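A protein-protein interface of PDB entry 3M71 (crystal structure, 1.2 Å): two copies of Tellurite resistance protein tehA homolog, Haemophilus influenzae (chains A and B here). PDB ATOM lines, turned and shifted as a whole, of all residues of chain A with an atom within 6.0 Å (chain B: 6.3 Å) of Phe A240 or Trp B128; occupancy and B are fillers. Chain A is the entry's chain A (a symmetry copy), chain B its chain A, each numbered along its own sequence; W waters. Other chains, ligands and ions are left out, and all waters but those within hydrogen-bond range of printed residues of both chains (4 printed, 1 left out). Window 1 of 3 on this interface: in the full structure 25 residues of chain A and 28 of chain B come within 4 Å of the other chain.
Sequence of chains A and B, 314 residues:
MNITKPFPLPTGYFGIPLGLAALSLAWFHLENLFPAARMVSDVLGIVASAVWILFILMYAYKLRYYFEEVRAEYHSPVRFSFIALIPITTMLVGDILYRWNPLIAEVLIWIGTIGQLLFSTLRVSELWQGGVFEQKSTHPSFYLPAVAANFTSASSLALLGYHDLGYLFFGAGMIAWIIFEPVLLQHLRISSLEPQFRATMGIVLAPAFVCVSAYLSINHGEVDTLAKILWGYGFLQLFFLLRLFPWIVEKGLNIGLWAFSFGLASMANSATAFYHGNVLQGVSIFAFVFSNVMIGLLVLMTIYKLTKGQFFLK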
ATOM      1  N   LEU A 185     -30.626  11.422 -12.045  1.00  0.00           N
ATOM      2  CA  LEU A 185     -29.944  10.572 -13.010  1.00  0.00           C
ATOM      3  C   LEU A 185     -29.332  11.399 -14.141  1.00  0.00           C
ATOM      4  O   LEU A 185     -28.268  11.065 -14.660  1.00  0.00           O
ATOM      5  CB  LEU A 185     -30.851   9.467 -13.532  1.00  0.00           C
ATOM      6  CG  LEU A 185     -31.421   8.528 -12.481  1.00  0.00           C
ATOM      7  CD1 LEU A 185     -32.158   7.360 -13.156  1.00  0.00           C
ATOM      8  CD2 LEU A 185     -30.354   7.998 -11.533  1.00  0.00           C
ATOM      9  N   LEU A 188     -26.079  12.667 -12.751  1.00  0.00           N
ATOM     10  CA  LEU A 188     -25.046  11.634 -12.716  1.00  0.00           C
ATOM     11  C   LEU A 188     -24.501  11.365 -14.106  1.00  0.00           C
ATOM     12  O   LEU A 188     -23.304  11.106 -14.286  1.00  0.00           O
ATOM     13  CB  LEU A 188     -25.573  10.354 -12.080  1.00  0.00           C
ATOM     14  CG  LEU A 188     -25.983  10.449 -10.618  1.00  0.00           C
ATOM     15  CD1 LEU A 188     -26.566   9.091 -10.210  1.00  0.00           C
ATOM     16  CD2 LEU A 188     -24.818  10.835  -9.745  1.00  0.00           C
ATOM     17  N   ARG A 189     -25.365  11.377 -15.125  1.00  0.00           N
ATOM     18  CA  ARG A 189     -24.898  11.169 -16.493  1.00  0.00           C
ATOM     19  C   ARG A 189     -23.899  12.231 -16.922  1.00  0.00           C
ATOM     20  O   ARG A 189     -22.922  11.912 -17.618  1.00  0.00           O
ATOM     21  CB  ARG A 189     -26.061  11.158 -17.507  1.00  0.00           C
ATOM     22  CG  ARG A 189     -26.911   9.888 -17.528  1.00  0.00           C
ATOM     23  CD  ARG A 189     -27.858   9.865 -18.719  1.00  0.00           C
ATOM     24  NE  ARG A 189     -29.045  10.740 -18.538  1.00  0.00           N
ATOM     25  CZ  ARG A 189     -30.156  10.359 -17.944  1.00  0.00           C
ATOM     26  NH1 ARG A 189     -30.304   9.114 -17.535  1.00  0.00           N
ATOM     27  NH2 ARG A 189     -31.155  11.214 -17.835  1.00  0.00           N
ATOM     28  N   SER A 191     -22.242  14.718 -14.878  1.00  0.00           N
ATOM     29  CA  SER A 191     -21.191  15.031 -13.912  1.00  0.00           C
ATOM     30  C   SER A 191     -20.709  13.774 -13.224  1.00  0.00           C
ATOM     31  O   SER A 191     -21.476  13.122 -12.555  1.00  0.00           O
ATOM     32  CB  SER A 191     -21.770  16.026 -12.896  1.00  0.00           C
ATOM     33  OG  SER A 191     -22.037  17.299 -13.505  1.00  0.00           O
ATOM     34  N   SER A 192     -19.423  13.432 -13.343  1.00  0.00           N
ATOM     35  CA  SER A 192     -18.905  12.328 -12.534  1.00  0.00           C
ATOM     36  C   SER A 192     -18.892  12.605 -11.059  1.00  0.00           C
ATOM     37  O   SER A 192     -18.119  13.440 -10.583  1.00  0.00           O
ATOM     38  CB  SER A 192     -17.475  11.936 -12.958  1.00  0.00           C
ATOM     39  OG  SER A 192     -17.463  11.551 -14.274  1.00  0.00           O
ATOM     40  N   LEU A 193     -19.609  11.794 -10.305  1.00  0.00           N
ATOM     41  CA  LEU A 193     -19.633  11.910  -8.871  1.00  0.00           C
ATOM     42  C   LEU A 193     -18.231  11.606  -8.374  1.00  0.00           C
ATOM     43  O   LEU A 193     -17.581  10.653  -8.823  1.00  0.00           O
ATOM     44  CB  LEU A 193     -20.701  10.936  -8.328  1.00  0.00           C
ATOM     45  CG  LEU A 193     -21.049  11.027  -6.825  1.00  0.00           C
ATOM     46  CD1 LEU A 193     -21.578  12.401  -6.464  1.00  0.00           C
ATOM     47  CD2 LEU A 193     -22.052   9.908  -6.437  1.00  0.00           C
ATOM     48  N   MET A 201     -23.991   6.119  -3.951  1.00  0.00           N
ATOM     49  CA  MET A 201     -24.718   5.491  -5.036  1.00  0.00           C
ATOM     50  C   MET A 201     -25.537   4.319  -4.545  1.00  0.00           C
ATOM     51  O   MET A 201     -26.565   3.981  -5.150  1.00  0.00           O
ATOM     52  CB  MET A 201     -23.775   5.000  -6.119  1.00  0.00           C
ATOM     53  CG  MET A 201     -23.167   6.121  -6.939  1.00  0.00           C
ATOM     54  SD  MET A 201     -24.310   7.100  -7.877  1.00  0.00           S
ATOM     55  CE  MET A 201     -24.874   5.871  -9.011  1.00  0.00           C
ATOM     56  N   VAL A 204     -29.235   4.865  -4.335  1.00  0.00           N
ATOM     57  CA  VAL A 204     -30.052   4.748  -5.543  1.00  0.00           C
ATOM     58  C   VAL A 204     -30.821   3.411  -5.614  1.00  0.00           C
ATOM     59  O   VAL A 204     -31.851   3.300  -6.251  1.00  0.00           O
ATOM     60  CB  VAL A 204     -29.193   5.001  -6.781  1.00  0.00           C
ATOM     61  CG1 VAL A 204     -29.982   4.833  -8.091  1.00  0.00           C
ATOM     62  CG2 VAL A 204     -28.565   6.398  -6.737  1.00  0.00           C
ATOM     63  N   TYR A 233     -38.643  -2.207 -11.608  1.00  0.00           N
ATOM     64  CA  TYR A 233     -37.698  -1.104 -11.655  1.00  0.00           C
ATOM     65  C   TYR A 233     -36.608  -1.273 -10.606  1.00  0.00           C
ATOM     66  O   TYR A 233     -35.454  -0.973 -10.837  1.00  0.00           O
ATOM     67  CB  TYR A 233     -38.414   0.237 -11.471  1.00  0.00           C
ATOM     68  CG  TYR A 233     -37.533   1.432 -11.750  1.00  0.00           C
ATOM     69  CD1 TYR A 233     -37.235   1.802 -13.028  1.00  0.00           C
ATOM     70  CD2 TYR A 233     -36.997   2.214 -10.725  1.00  0.00           C
ATOM     71  CE1 TYR A 233     -36.462   2.922 -13.302  1.00  0.00           C
ATOM     72  CE2 TYR A 233     -36.193   3.306 -10.997  1.00  0.00           C
ATOM     73  CZ  TYR A 233     -35.944   3.661 -12.304  1.00  0.00           C
ATOM     74  OH  TYR A 233     -35.185   4.771 -12.619  1.00  0.00           O
ATOM     75  N   PHE A 235     -35.234  -4.055  -9.565  1.00  0.00           N
ATOM     76  CA  PHE A 235     -34.233  -4.969 -10.088  1.00  0.00           C
ATOM     77  C   PHE A 235     -33.409  -4.362 -11.211  1.00  0.00           C
ATOM     78  O   PHE A 235     -32.212  -4.642 -11.310  1.00  0.00           O
ATOM     79  CB  PHE A 235     -34.838  -6.313 -10.539  1.00  0.00           C
ATOM     80  CG  PHE A 235     -35.239  -7.176  -9.380  1.00  0.00           C
ATOM     81  CD1 PHE A 235     -34.333  -7.543  -8.448  1.00  0.00           C
ATOM     82  CD2 PHE A 235     -36.532  -7.579  -9.207  1.00  0.00           C
ATOM     83  CE1 PHE A 235     -34.697  -8.354  -7.384  1.00  0.00           C
ATOM     84  CE2 PHE A 235     -36.896  -8.384  -8.132  1.00  0.00           C
ATOM     85  CZ  PHE A 235     -35.979  -8.669  -7.242  1.00  0.00           C
ATOM     86  N   LEU A 236     -34.019  -3.557 -12.073  1.00  0.00           N
ATOM     87  CA  LEU A 236     -33.247  -2.822 -13.069  1.00  0.00           C
ATOM     88  C   LEU A 236     -32.146  -2.036 -12.422  1.00  0.00           C
ATOM     89  O   LEU A 236     -30.989  -2.090 -12.834  1.00  0.00           O
ATOM     90  CB  LEU A 236     -34.195  -1.877 -13.864  1.00  0.00           C
ATOM     91  CG  LEU A 236     -33.541  -1.118 -15.016  1.00  0.00           C
ATOM     92  CD1 LEU A 236     -33.347  -2.029 -16.194  1.00  0.00           C
ATOM     93  CD2 LEU A 236     -34.354   0.106 -15.384  1.00  0.00           C
ATOM     94  N   GLN A 237     -32.484  -1.274 -11.382  1.00  0.00           N
ATOM     95  CA  GLN A 237     -31.502  -0.444 -10.679  1.00  0.00           C
ATOM     96  C   GLN A 237     -30.454  -1.306 -10.001  1.00  0.00           C
ATOM     97  O   GLN A 237     -29.264  -0.955 -10.011  1.00  0.00           O
ATOM     98  CB  GLN A 237     -32.197   0.473  -9.665  1.00  0.00           C
ATOM     99  CG  GLN A 237     -33.230   1.461 -10.217  1.00  0.00           C
ATOM    100  CD  GLN A 237     -32.655   2.459 -11.164  1.00  0.00           C
ATOM    101  OE1 GLN A 237     -32.238   2.133 -12.267  1.00  0.00           O
ATOM    102  NE2 GLN A 237     -32.604   3.737 -10.712  1.00  0.00           N
ATOM    103  N   LEU A 238     -30.860  -2.432  -9.449  1.00  0.00           N
ATOM    104  CA  LEU A 238     -29.883  -3.363  -8.874  1.00  0.00           C
ATOM    105  C   LEU A 238     -28.853  -3.792  -9.918  1.00  0.00           C
ATOM    106  O   LEU A 238     -27.624  -3.824  -9.664  1.00  0.00           O
ATOM    107  CB  LEU A 238     -30.595  -4.596  -8.305  1.00  0.00           C
ATOM    108  CG  LEU A 238     -29.660  -5.656  -7.748  1.00  0.00           C
ATOM    109  CD1 LEU A 238     -28.832  -5.202  -6.631  1.00  0.00           C
ATOM    110  CD2 LEU A 238     -30.465  -6.939  -7.424  1.00  0.00           C
ATOM    111  N   PHE A 239     -29.327  -4.227 -11.081  1.00  0.00           N
ATOM    112  CA  PHE A 239     -28.420  -4.667 -12.126  1.00  0.00           C
ATOM    113  C   PHE A 239     -27.478  -3.543 -12.552  1.00  0.00           C
ATOM    114  O   PHE A 239     -26.280  -3.790 -12.781  1.00  0.00           O
ATOM    115  CB  PHE A 239     -29.157  -5.206 -13.340  1.00  0.00           C
ATOM    116  CG  PHE A 239     -30.005  -6.411 -13.080  1.00  0.00           C
ATOM    117  CD1 PHE A 239     -29.859  -7.211 -11.975  1.00  0.00           C
ATOM    118  CD2 PHE A 239     -31.093  -6.628 -13.860  1.00  0.00           C
ATOM    119  CE1 PHE A 239     -30.690  -8.302 -11.786  1.00  0.00           C
ATOM    120  CE2 PHE A 239     -31.910  -7.701 -13.669  1.00  0.00           C
ATOM    121  CZ  PHE A 239     -31.690  -8.521 -12.623  1.00  0.00           C
ATOM    122  N   PHE A 240     -28.004  -2.344 -12.716  1.00  0.00           N
ATOM    123  CA  PHE A 240     -27.175  -1.189 -13.073  1.00  0.00           C
ATOM    124  C   PHE A 240     -26.101  -0.944 -12.016  1.00  0.00           C
ATOM    125  O   PHE A 240     -24.925  -0.729 -12.360  1.00  0.00           O
ATOM    126  CB  PHE A 240     -28.060   0.053 -13.209  1.00  0.00           C
ATOM    127  CG  PHE A 240     -28.900   0.131 -14.464  1.00  0.00           C
ATOM    128  CD1 PHE A 240     -29.018  -0.920 -15.388  1.00  0.00           C
ATOM    129  CD2 PHE A 240     -29.656   1.263 -14.722  1.00  0.00           C
ATOM    130  CE1 PHE A 240     -29.781  -0.788 -16.532  1.00  0.00           C
ATOM    131  CE2 PHE A 240     -30.429   1.364 -15.849  1.00  0.00           C
ATOM    132  CZ  PHE A 240     -30.481   0.374 -16.759  1.00  0.00           C
ATOM    133  N   LEU A 241     -26.475  -0.993 -10.733  1.00  0.00           N
ATOM    134  CA  LEU A 241     -25.507  -0.730  -9.664  1.00  0.00           C
ATOM    135  C   LEU A 241     -24.482  -1.849  -9.535  1.00  0.00           C
ATOM    136  O   LEU A 241     -23.319  -1.599  -9.228  1.00  0.00           O
ATOM    137  CB  LEU A 241     -26.235  -0.490  -8.359  1.00  0.00           C
ATOM    138  CG  LEU A 241     -26.994   0.841  -8.331  1.00  0.00           C
ATOM    139  CD1 LEU A 241     -28.000   0.875  -7.204  1.00  0.00           C
ATOM    140  CD2 LEU A 241     -26.042   2.010  -8.241  1.00  0.00           C
ATOM    141  N   LEU A 242     -24.884  -3.096  -9.816  1.00  0.00           N
ATOM    142  CA  LEU A 242     -23.910  -4.189  -9.853  1.00  0.00           C
ATOM    143  C   LEU A 242     -22.874  -3.941 -10.944  1.00  0.00           C
ATOM    144  O   LEU A 242     -21.664  -4.085 -10.711  1.00  0.00           O
ATOM    145  CB  LEU A 242     -24.609  -5.513 -10.063  1.00  0.00           C
ATOM    146  CG  LEU A 242     -25.347  -6.123  -8.910  1.00  0.00           C
ATOM    147  CD1 LEU A 242     -26.225  -7.256  -9.325  1.00  0.00           C
ATOM    148  CD2 LEU A 242     -24.402  -6.621  -7.857  1.00  0.00           C
ATOM    149  N   ARG A 243     -23.312  -3.528 -12.135  1.00  0.00           N
ATOM    150  CA  ARG A 243     -22.363  -3.246 -13.191  1.00  0.00           C
ATOM    151  C   ARG A 243     -21.431  -2.081 -12.804  1.00  0.00           C
ATOM    152  O   ARG A 243     -20.253  -2.090 -13.154  1.00  0.00           O
ATOM    153  CB  ARG A 243     -23.122  -2.967 -14.478  1.00  0.00           C
ATOM    154  CG  ARG A 243     -22.279  -2.804 -15.711  1.00  0.00           C
ATOM    155  CD  ARG A 243     -21.797  -1.369 -15.978  1.00  0.00           C
ATOM    156  NE  ARG A 243     -21.188  -1.241 -17.310  1.00  0.00           N
ATOM    157  CZ  ARG A 243     -19.930  -1.429 -17.553  1.00  0.00           C
ATOM    158  NH1 ARG A 243     -19.120  -1.700 -16.537  1.00  0.00           N
ATOM    159  NH2 ARG A 243     -19.482  -1.315 -18.792  1.00  0.00           N
ATOM    160  N   LEU A 244     -21.985  -1.107 -12.107  1.00  0.00           N
ATOM    161  CA  LEU A 244     -21.256   0.064 -11.664  1.00  0.00           C
ATOM    162  C   LEU A 244     -20.358  -0.169 -10.447  1.00  0.00           C
ATOM    163  O   LEU A 244     -19.584   0.737 -10.056  1.00  0.00           O
ATOM    164  CB  LEU A 244     -22.216   1.200 -11.374  1.00  0.00           C
ATOM    165  CG  LEU A 244     -22.846   1.868 -12.601  1.00  0.00           C
ATOM    166  CD1 LEU A 244     -24.034   2.686 -12.164  1.00  0.00           C
ATOM    167  CD2 LEU A 244     -21.831   2.688 -13.392  1.00  0.00           C
ATOM    168  N   PHE A 245     -20.445  -1.338  -9.812  1.00  0.00           N
ATOM    169  CA  PHE A 245     -19.803  -1.488  -8.519  1.00  0.00           C
ATOM    170  C   PHE A 245     -18.278  -1.265  -8.571  1.00  0.00           C
ATOM    171  O   PHE A 245     -17.730  -0.591  -7.697  1.00  0.00           O
ATOM    172  CB  PHE A 245     -20.166  -2.842  -7.864  1.00  0.00           C
ATOM    173  CG  PHE A 245     -19.803  -2.880  -6.411  1.00  0.00           C
ATOM    174  CD1 PHE A 245     -20.631  -2.313  -5.462  1.00  0.00           C
ATOM    175  CD2 PHE A 245     -18.622  -3.473  -5.992  1.00  0.00           C
ATOM    176  CE1 PHE A 245     -20.312  -2.346  -4.118  1.00  0.00           C
ATOM    177  CE2 PHE A 245     -18.295  -3.493  -4.637  1.00  0.00           C
ATOM    178  CZ  PHE A 245     -19.145  -2.945  -3.722  1.00  0.00           C
ATOM    179  N   TRP A 247     -16.561   0.764 -10.412  1.00  0.00           N
ATOM    180  CA  TRP A 247     -16.416   2.216 -10.423  1.00  0.00           C
ATOM    181  C   TRP A 247     -16.753   2.842  -9.085  1.00  0.00           C
ATOM    182  O   TRP A 247     -16.039   3.731  -8.598  1.00  0.00           O
ATOM    183  CB  TRP A 247     -17.263   2.838 -11.541  1.00  0.00           C
ATOM    184  CG  TRP A 247     -17.402   4.348 -11.575  1.00  0.00           C
ATOM    185  CD1 TRP A 247     -16.534   5.250 -12.177  1.00  0.00           C
ATOM    186  CD2 TRP A 247     -18.486   5.143 -11.070  1.00  0.00           C
ATOM    187  NE1 TRP A 247     -17.002   6.525 -12.039  1.00  0.00           N
ATOM    188  CE2 TRP A 247     -18.181   6.500 -11.342  1.00  0.00           C
ATOM    189  CE3 TRP A 247     -19.692   4.852 -10.408  1.00  0.00           C
ATOM    190  CZ2 TRP A 247     -19.034   7.532 -10.987  1.00  0.00           C
ATOM    191  CZ3 TRP A 247     -20.504   5.884 -10.057  1.00  0.00           C
ATOM    192  CH2 TRP A 247     -20.186   7.196 -10.345  1.00  0.00           C
ATOM    193  N   LEU B 117     -31.584  -6.688 -22.071  1.00  0.00           N
ATOM    194  CA  LEU B 117     -31.261  -6.448 -20.679  1.00  0.00           C
ATOM    195  C   LEU B 117     -29.763  -6.370 -20.454  1.00  0.00           C
ATOM    196  O   LEU B 117     -29.276  -5.531 -19.689  1.00  0.00           O
ATOM    197  CB  LEU B 117     -31.895  -7.544 -19.809  1.00  0.00           C
ATOM    198  CG  LEU B 117     -31.728  -7.370 -18.329  1.00  0.00           C
ATOM    199  CD1 LEU B 117     -32.282  -6.048 -17.746  1.00  0.00           C
ATOM    200  CD2 LEU B 117     -32.351  -8.599 -17.589  1.00  0.00           C
ATOM    201  N   SER B 120     -28.606  -2.848 -21.887  1.00  0.00           N
ATOM    202  CA  SER B 120     -28.879  -1.726 -20.987  1.00  0.00           C
ATOM    203  C   SER B 120     -28.032  -1.777 -19.739  1.00  0.00           C
ATOM    204  O   SER B 120     -27.495  -0.754 -19.286  1.00  0.00           O
ATOM    205  CB  SER B 120     -30.359  -1.694 -20.628  1.00  0.00           C
ATOM    206  OG  SER B 120     -30.710  -2.726 -19.732  1.00  0.00           O
ATOM    207  N   THR B 121     -27.916  -2.967 -19.160  1.00  0.00           N
ATOM    208  CA  THR B 121     -27.107  -3.134 -17.989  1.00  0.00           C
ATOM    209  C   THR B 121     -25.668  -2.713 -18.252  1.00  0.00           C
ATOM    210  O   THR B 121     -25.010  -2.132 -17.357  1.00  0.00           O
ATOM    211  CB  THR B 121     -27.168  -4.586 -17.472  1.00  0.00           C
ATOM    212  OG1 THR B 121     -28.512  -4.856 -17.040  1.00  0.00           O
ATOM    213  CG2 THR B 121     -26.250  -4.805 -16.315  1.00  0.00           C
ATOM    214  N   LEU B 122     -25.140  -3.040 -19.418  1.00  0.00           N
ATOM    215  CA  LEU B 122     -23.786  -2.609 -19.736  1.00  0.00           C
ATOM    216  C   LEU B 122     -23.663  -1.127 -20.065  1.00  0.00           C
ATOM    217  O   LEU B 122     -22.721  -0.478 -19.615  1.00  0.00           O
ATOM    218  CB  LEU B 122     -23.250  -3.413 -20.915  1.00  0.00           C
ATOM    219  CG  LEU B 122     -22.938  -4.883 -20.633  1.00  0.00           C
ATOM    220  CD1 LEU B 122     -22.680  -5.674 -21.905  1.00  0.00           C
ATOM    221  CD2 LEU B 122     -21.801  -4.998 -19.701  1.00  0.00           C
ATOM    222  N   ARG B 123     -24.580  -0.576 -20.859  1.00  0.00           N
ATOM    223  CA  ARG B 123     -24.442   0.789 -21.395  1.00  0.00           C
ATOM    224  C   ARG B 123     -25.248   1.885 -20.778  1.00  0.00           C
ATOM    225  O   ARG B 123     -24.733   2.994 -20.604  1.00  0.00           O
ATOM    226  CB  ARG B 123     -24.710   0.774 -22.883  1.00  0.00           C
ATOM    227  CG  ARG B 123     -23.613   0.098 -23.588  1.00  0.00           C
ATOM    228  CD  ARG B 123     -22.289   0.890 -23.521  1.00  0.00           C
ATOM    229  NE  ARG B 123     -22.437   2.146 -24.260  1.00  0.00           N
ATOM    230  CZ  ARG B 123     -22.283   3.374 -23.773  1.00  0.00           C
ATOM    231  NH1 ARG B 123     -21.841   3.591 -22.541  1.00  0.00           N
ATOM    232  NH2 ARG B 123     -22.528   4.404 -24.564  1.00  0.00           N
ATOM    233  N   VAL B 124     -26.497   1.624 -20.459  1.00  0.00           N
ATOM    234  CA  VAL B 124     -27.339   2.674 -19.855  1.00  0.00           C
ATOM    235  C   VAL B 124     -26.765   3.044 -18.479  1.00  0.00           C
ATOM    236  O   VAL B 124     -26.668   4.235 -18.142  1.00  0.00           O
ATOM    237  CB  VAL B 124     -28.822   2.270 -19.796  1.00  0.00           C
ATOM    238  CG1 VAL B 124     -29.633   3.336 -19.002  1.00  0.00           C
ATOM    239  CG2 VAL B 124     -29.397   2.143 -21.198  1.00  0.00           C
ATOM    240  N   SER B 125     -26.379   2.020 -17.697  1.00  0.00           N
ATOM    241  CA  SER B 125     -25.794   2.260 -16.380  1.00  0.00           C
ATOM    242  C   SER B 125     -24.453   2.992 -16.484  1.00  0.00           C
ATOM    243  O   SER B 125     -24.133   3.828 -15.632  1.00  0.00           O
ATOM    244  CB  SER B 125     -25.605   0.965 -15.619  1.00  0.00           C
ATOM    245  OG  SER B 125     -24.590   0.217 -16.238  1.00  0.00           O
ATOM    246  N   GLU B 126     -23.662   2.648 -17.506  1.00  0.00           N
ATOM    247  CA  GLU B 126     -22.325   3.220 -17.632  1.00  0.00           C
ATOM    248  C   GLU B 126     -22.386   4.743 -17.755  1.00  0.00           C
ATOM    249  O   GLU B 126     -21.446   5.447 -17.350  1.00  0.00           O
ATOM    250  CB  GLU B 126     -21.606   2.624 -18.848  1.00  0.00           C
ATOM    251  CG  GLU B 126     -20.191   2.977 -18.975  1.00  0.00           C
ATOM    252  CD  GLU B 126     -19.495   2.239 -20.085  1.00  0.00           C
ATOM    253  OE1 GLU B 126     -20.104   1.808 -21.098  1.00  0.00           O
ATOM    254  OE2 GLU B 126     -18.237   2.084 -19.968  1.00  0.00           O
ATOM    255  N   LEU B 127     -23.450   5.239 -18.349  1.00  0.00           N
ATOM    256  CA  LEU B 127     -23.629   6.696 -18.480  1.00  0.00           C
ATOM    257  C   LEU B 127     -23.557   7.389 -17.115  1.00  0.00           C
ATOM    258  O   LEU B 127     -23.112   8.542 -17.027  1.00  0.00           O
ATOM    259  CB  LEU B 127     -24.957   7.043 -19.187  1.00  0.00           C
ATOM    260  CG  LEU B 127     -25.101   6.454 -20.587  1.00  0.00           C
ATOM    261  CD1 LEU B 127     -26.506   6.786 -21.098  1.00  0.00           C
ATOM    262  CD2 LEU B 127     -24.065   6.984 -21.558  1.00  0.00           C
ATOM    263  N   TRP B 128     -24.004   6.717 -16.033  1.00  0.00           N
ATOM    264  CA  TRP B 128     -24.047   7.298 -14.708  1.00  0.00           C
ATOM    265  C   TRP B 128     -22.676   7.555 -14.139  1.00  0.00           C
ATOM    266  O   TRP B 128     -22.553   8.143 -13.082  1.00  0.00           O
ATOM    267  CB  TRP B 128     -24.826   6.422 -13.717  1.00  0.00           C
ATOM    268  CG  TRP B 128     -26.276   6.178 -13.954  1.00  0.00           C
ATOM    269  CD1 TRP B 128     -27.086   6.558 -15.005  1.00  0.00           C
ATOM    270  CD2 TRP B 128     -27.091   5.375 -13.116  1.00  0.00           C
ATOM    271  NE1 TRP B 128     -28.369   6.058 -14.840  1.00  0.00           N
ATOM    272  CE2 TRP B 128     -28.386   5.295 -13.707  1.00  0.00           C
ATOM    273  CE3 TRP B 128     -26.845   4.647 -11.952  1.00  0.00           C
ATOM    274  CZ2 TRP B 128     -29.409   4.602 -13.120  1.00  0.00           C
ATOM    275  CZ3 TRP B 128     -27.866   3.944 -11.388  1.00  0.00           C
ATOM    276  CH2 TRP B 128     -29.142   3.920 -11.981  1.00  0.00           C
ATOM    277  N   GLN B 129     -21.597   7.079 -14.787  1.00  0.00           N
ATOM    278  CA  GLN B 129     -20.234   7.412 -14.392  1.00  0.00           C
ATOM    279  C   GLN B 129     -19.834   8.848 -14.693  1.00  0.00           C
ATOM    280  O   GLN B 129     -18.835   9.323 -14.164  1.00  0.00           O
ATOM    281  CB  GLN B 129     -19.228   6.476 -15.060  1.00  0.00           C
ATOM    282  CG  GLN B 129     -19.438   5.014 -14.727  1.00  0.00           C
ATOM    283  CD  GLN B 129     -18.456   4.077 -15.422  1.00  0.00           C
ATOM    284  OE1 GLN B 129     -17.706   4.496 -16.353  1.00  0.00           O
ATOM    285  NE2 GLN B 129     -18.489   2.817 -15.058  1.00  0.00           N
ATOM    286  N   GLY B 130     -20.597   9.520 -15.541  1.00  0.00           N
ATOM    287  CA  GLY B 130     -20.395  10.923 -15.826  1.00  0.00           C
ATOM    288  C   GLY B 130     -19.318  11.204 -16.852  1.00  0.00           C
ATOM    289  O   GLY B 130     -18.430  10.408 -17.121  1.00  0.00           O
HETATM  290  O   HOH W   1     -28.640   6.547 -18.023  1.00  0.00           O
HETATM  291  O   HOH W   2     -15.758   8.567 -13.625  1.00  0.00           O
HETATM  292  O   HOH W   3     -18.207   0.012 -13.275  1.00  0.00           O
HETATM  293  O   HOH W   4     -31.021   5.942 -16.628  1.00  0.00           O
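O of Leu B117 sits at hydrogen-bond distance from OG of Ser B120, at 3.2 Å. The side-chain hydroxyl of Thr B121 sits at hydrogen-bond distance from the backbone carbonyl oxygen of Leu B117, 2.8 Å away. The backbone NH of Ser B125 sits at hydrogen-bond distance from the backbone carbonyl oxygen of Ser B120 (3.4 Å). O of Thr B121 is in hydrogen-bond range of OG of Ser B125 (2.6 Å). The guanidinium group of Arg B123 is in salt-bridge range of the side-chain carboxylate of Glu B126 (2.9 Å). OH of Tyr A233 lies within hydrogen-bond range of NE2 of Gln A237 (3.4 Å).
No position is printed for both chains. Of the 26 pairs that touch across the chains among the printed residues, none has its exchanged pair printed and touching as well.
Hydrophobic or aromatic side chains of chain B that line the printed part of chain A: Val B124, Leu B127 and Trp B128. Of the 21 printed residues of chain A, 12 touch a printed residue of chain B. Hydrophobic or aromatic side chains of chain A within 4 Å of the printed part of chain B: Leu A185, Leu A188, Met A201, Phe A239, Phe A240, Leu A244 and Trp A247. Among the printed residues, 26 pairs touch across the chains. Among the printed residues, Asp or Glu carboxylates within 4 Å of a Lys or Arg side-chain nitrogen of the other chain: Arg A243 with Glu B126.
The backbone carbonyl oxygen (O) of Leu B122 sits at hydrogen-bond distance from the guanidinium group (NE) of Arg A243 (2.9 Å). The side-chain carboxylate (OE2) of Glu B126 is in salt-bridge range of the guanidinium group (NH2) of Arg A243, 3.8 Å away. The backbone carbonyl oxygen of Gln B129 lies within hydrogen-bond range of the side-chain hydroxyl of Ser A192 (2.6 Å). The backbone NH (N) of Gly B130 lies close to the backbone carbonyl oxygen (O) of Leu A188 (3.4 Å). O of Gly B130 sits close to OG of Ser A192. The backbone carbonyl oxygen (O) of Leu A188 lies close to the backbone carbonyl oxygen (O) of Trp B128, 3.3 Å away. The backbone carbonyl oxygen of Arg A189 sits close to the backbone carbonyl oxygen of Leu B127 (3.4 Å).
O of Arg A189 touches CA of Gly B130, 3.3 Å away. C of Ser A191 touches CA of Gly B130, 3.9 Å away. Met A201 touches Trp B128. OE1 of Gln A237 touches CH2 of Trp B128, 3.6 Å away. Phe A239 touches Thr B121. Val B124 touches Phe A240. Arg A243 touches Ser B125 (CD to OG, 3.2 Å). Leu A244 touches Trp B128 (CD1 to CE3, 3.4 Å). Leu A244 touches Gln B129 (CD2 to CG, 3.6 Å). Trp A247 touches Trp B128.
Water W2 lies within hydrogen-bond range of the indole nitrogen (NE1) of Trp A247 (2.9 Å), the backbone carbonyl oxygen (O) of Gln B129 (3.2 Å) and the side-chain hydroxyl (OG) of Ser A192 (3.5 Å). Water W3 lies within hydrogen-bond range of O of Arg A243 (2.9 Å), NE2 of Gln B129 (3.3 Å) and N of Trp A247 (3.4 Å). Water W1 lies within hydrogen-bond range of O of Val B124, NH1 of Arg A189 and NE1 of Trp B128. Water W4 lies within hydrogen-bond range of the indole nitrogen of Trp B128 (3.2 Å) and the guanidinium group of Arg A189 (3.4 Å).
Of the printed residues of chain B, Phe A240 touches Ser B120 (3.6 Å), Thr B121 (3.8 Å), Val B124 (3.8 Å), Ser B125 (3.6 Å) and Trp B128 (3.7 Å). Printed residues of chain A within 4 Å of Trp B128: Leu A185, Leu A188, Met A201, Gln A237, Phe A240, Leu A244 and Trp A247. Printed residues of chain B within 4 Å of Trp A247: Trp B128 (3.7 Å) and Gln B129 (3.6 Å). Printed residues of chain B within 4 Å of Gln A237: Trp B128. Phe A245 touches none of the printed residues of chain B.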
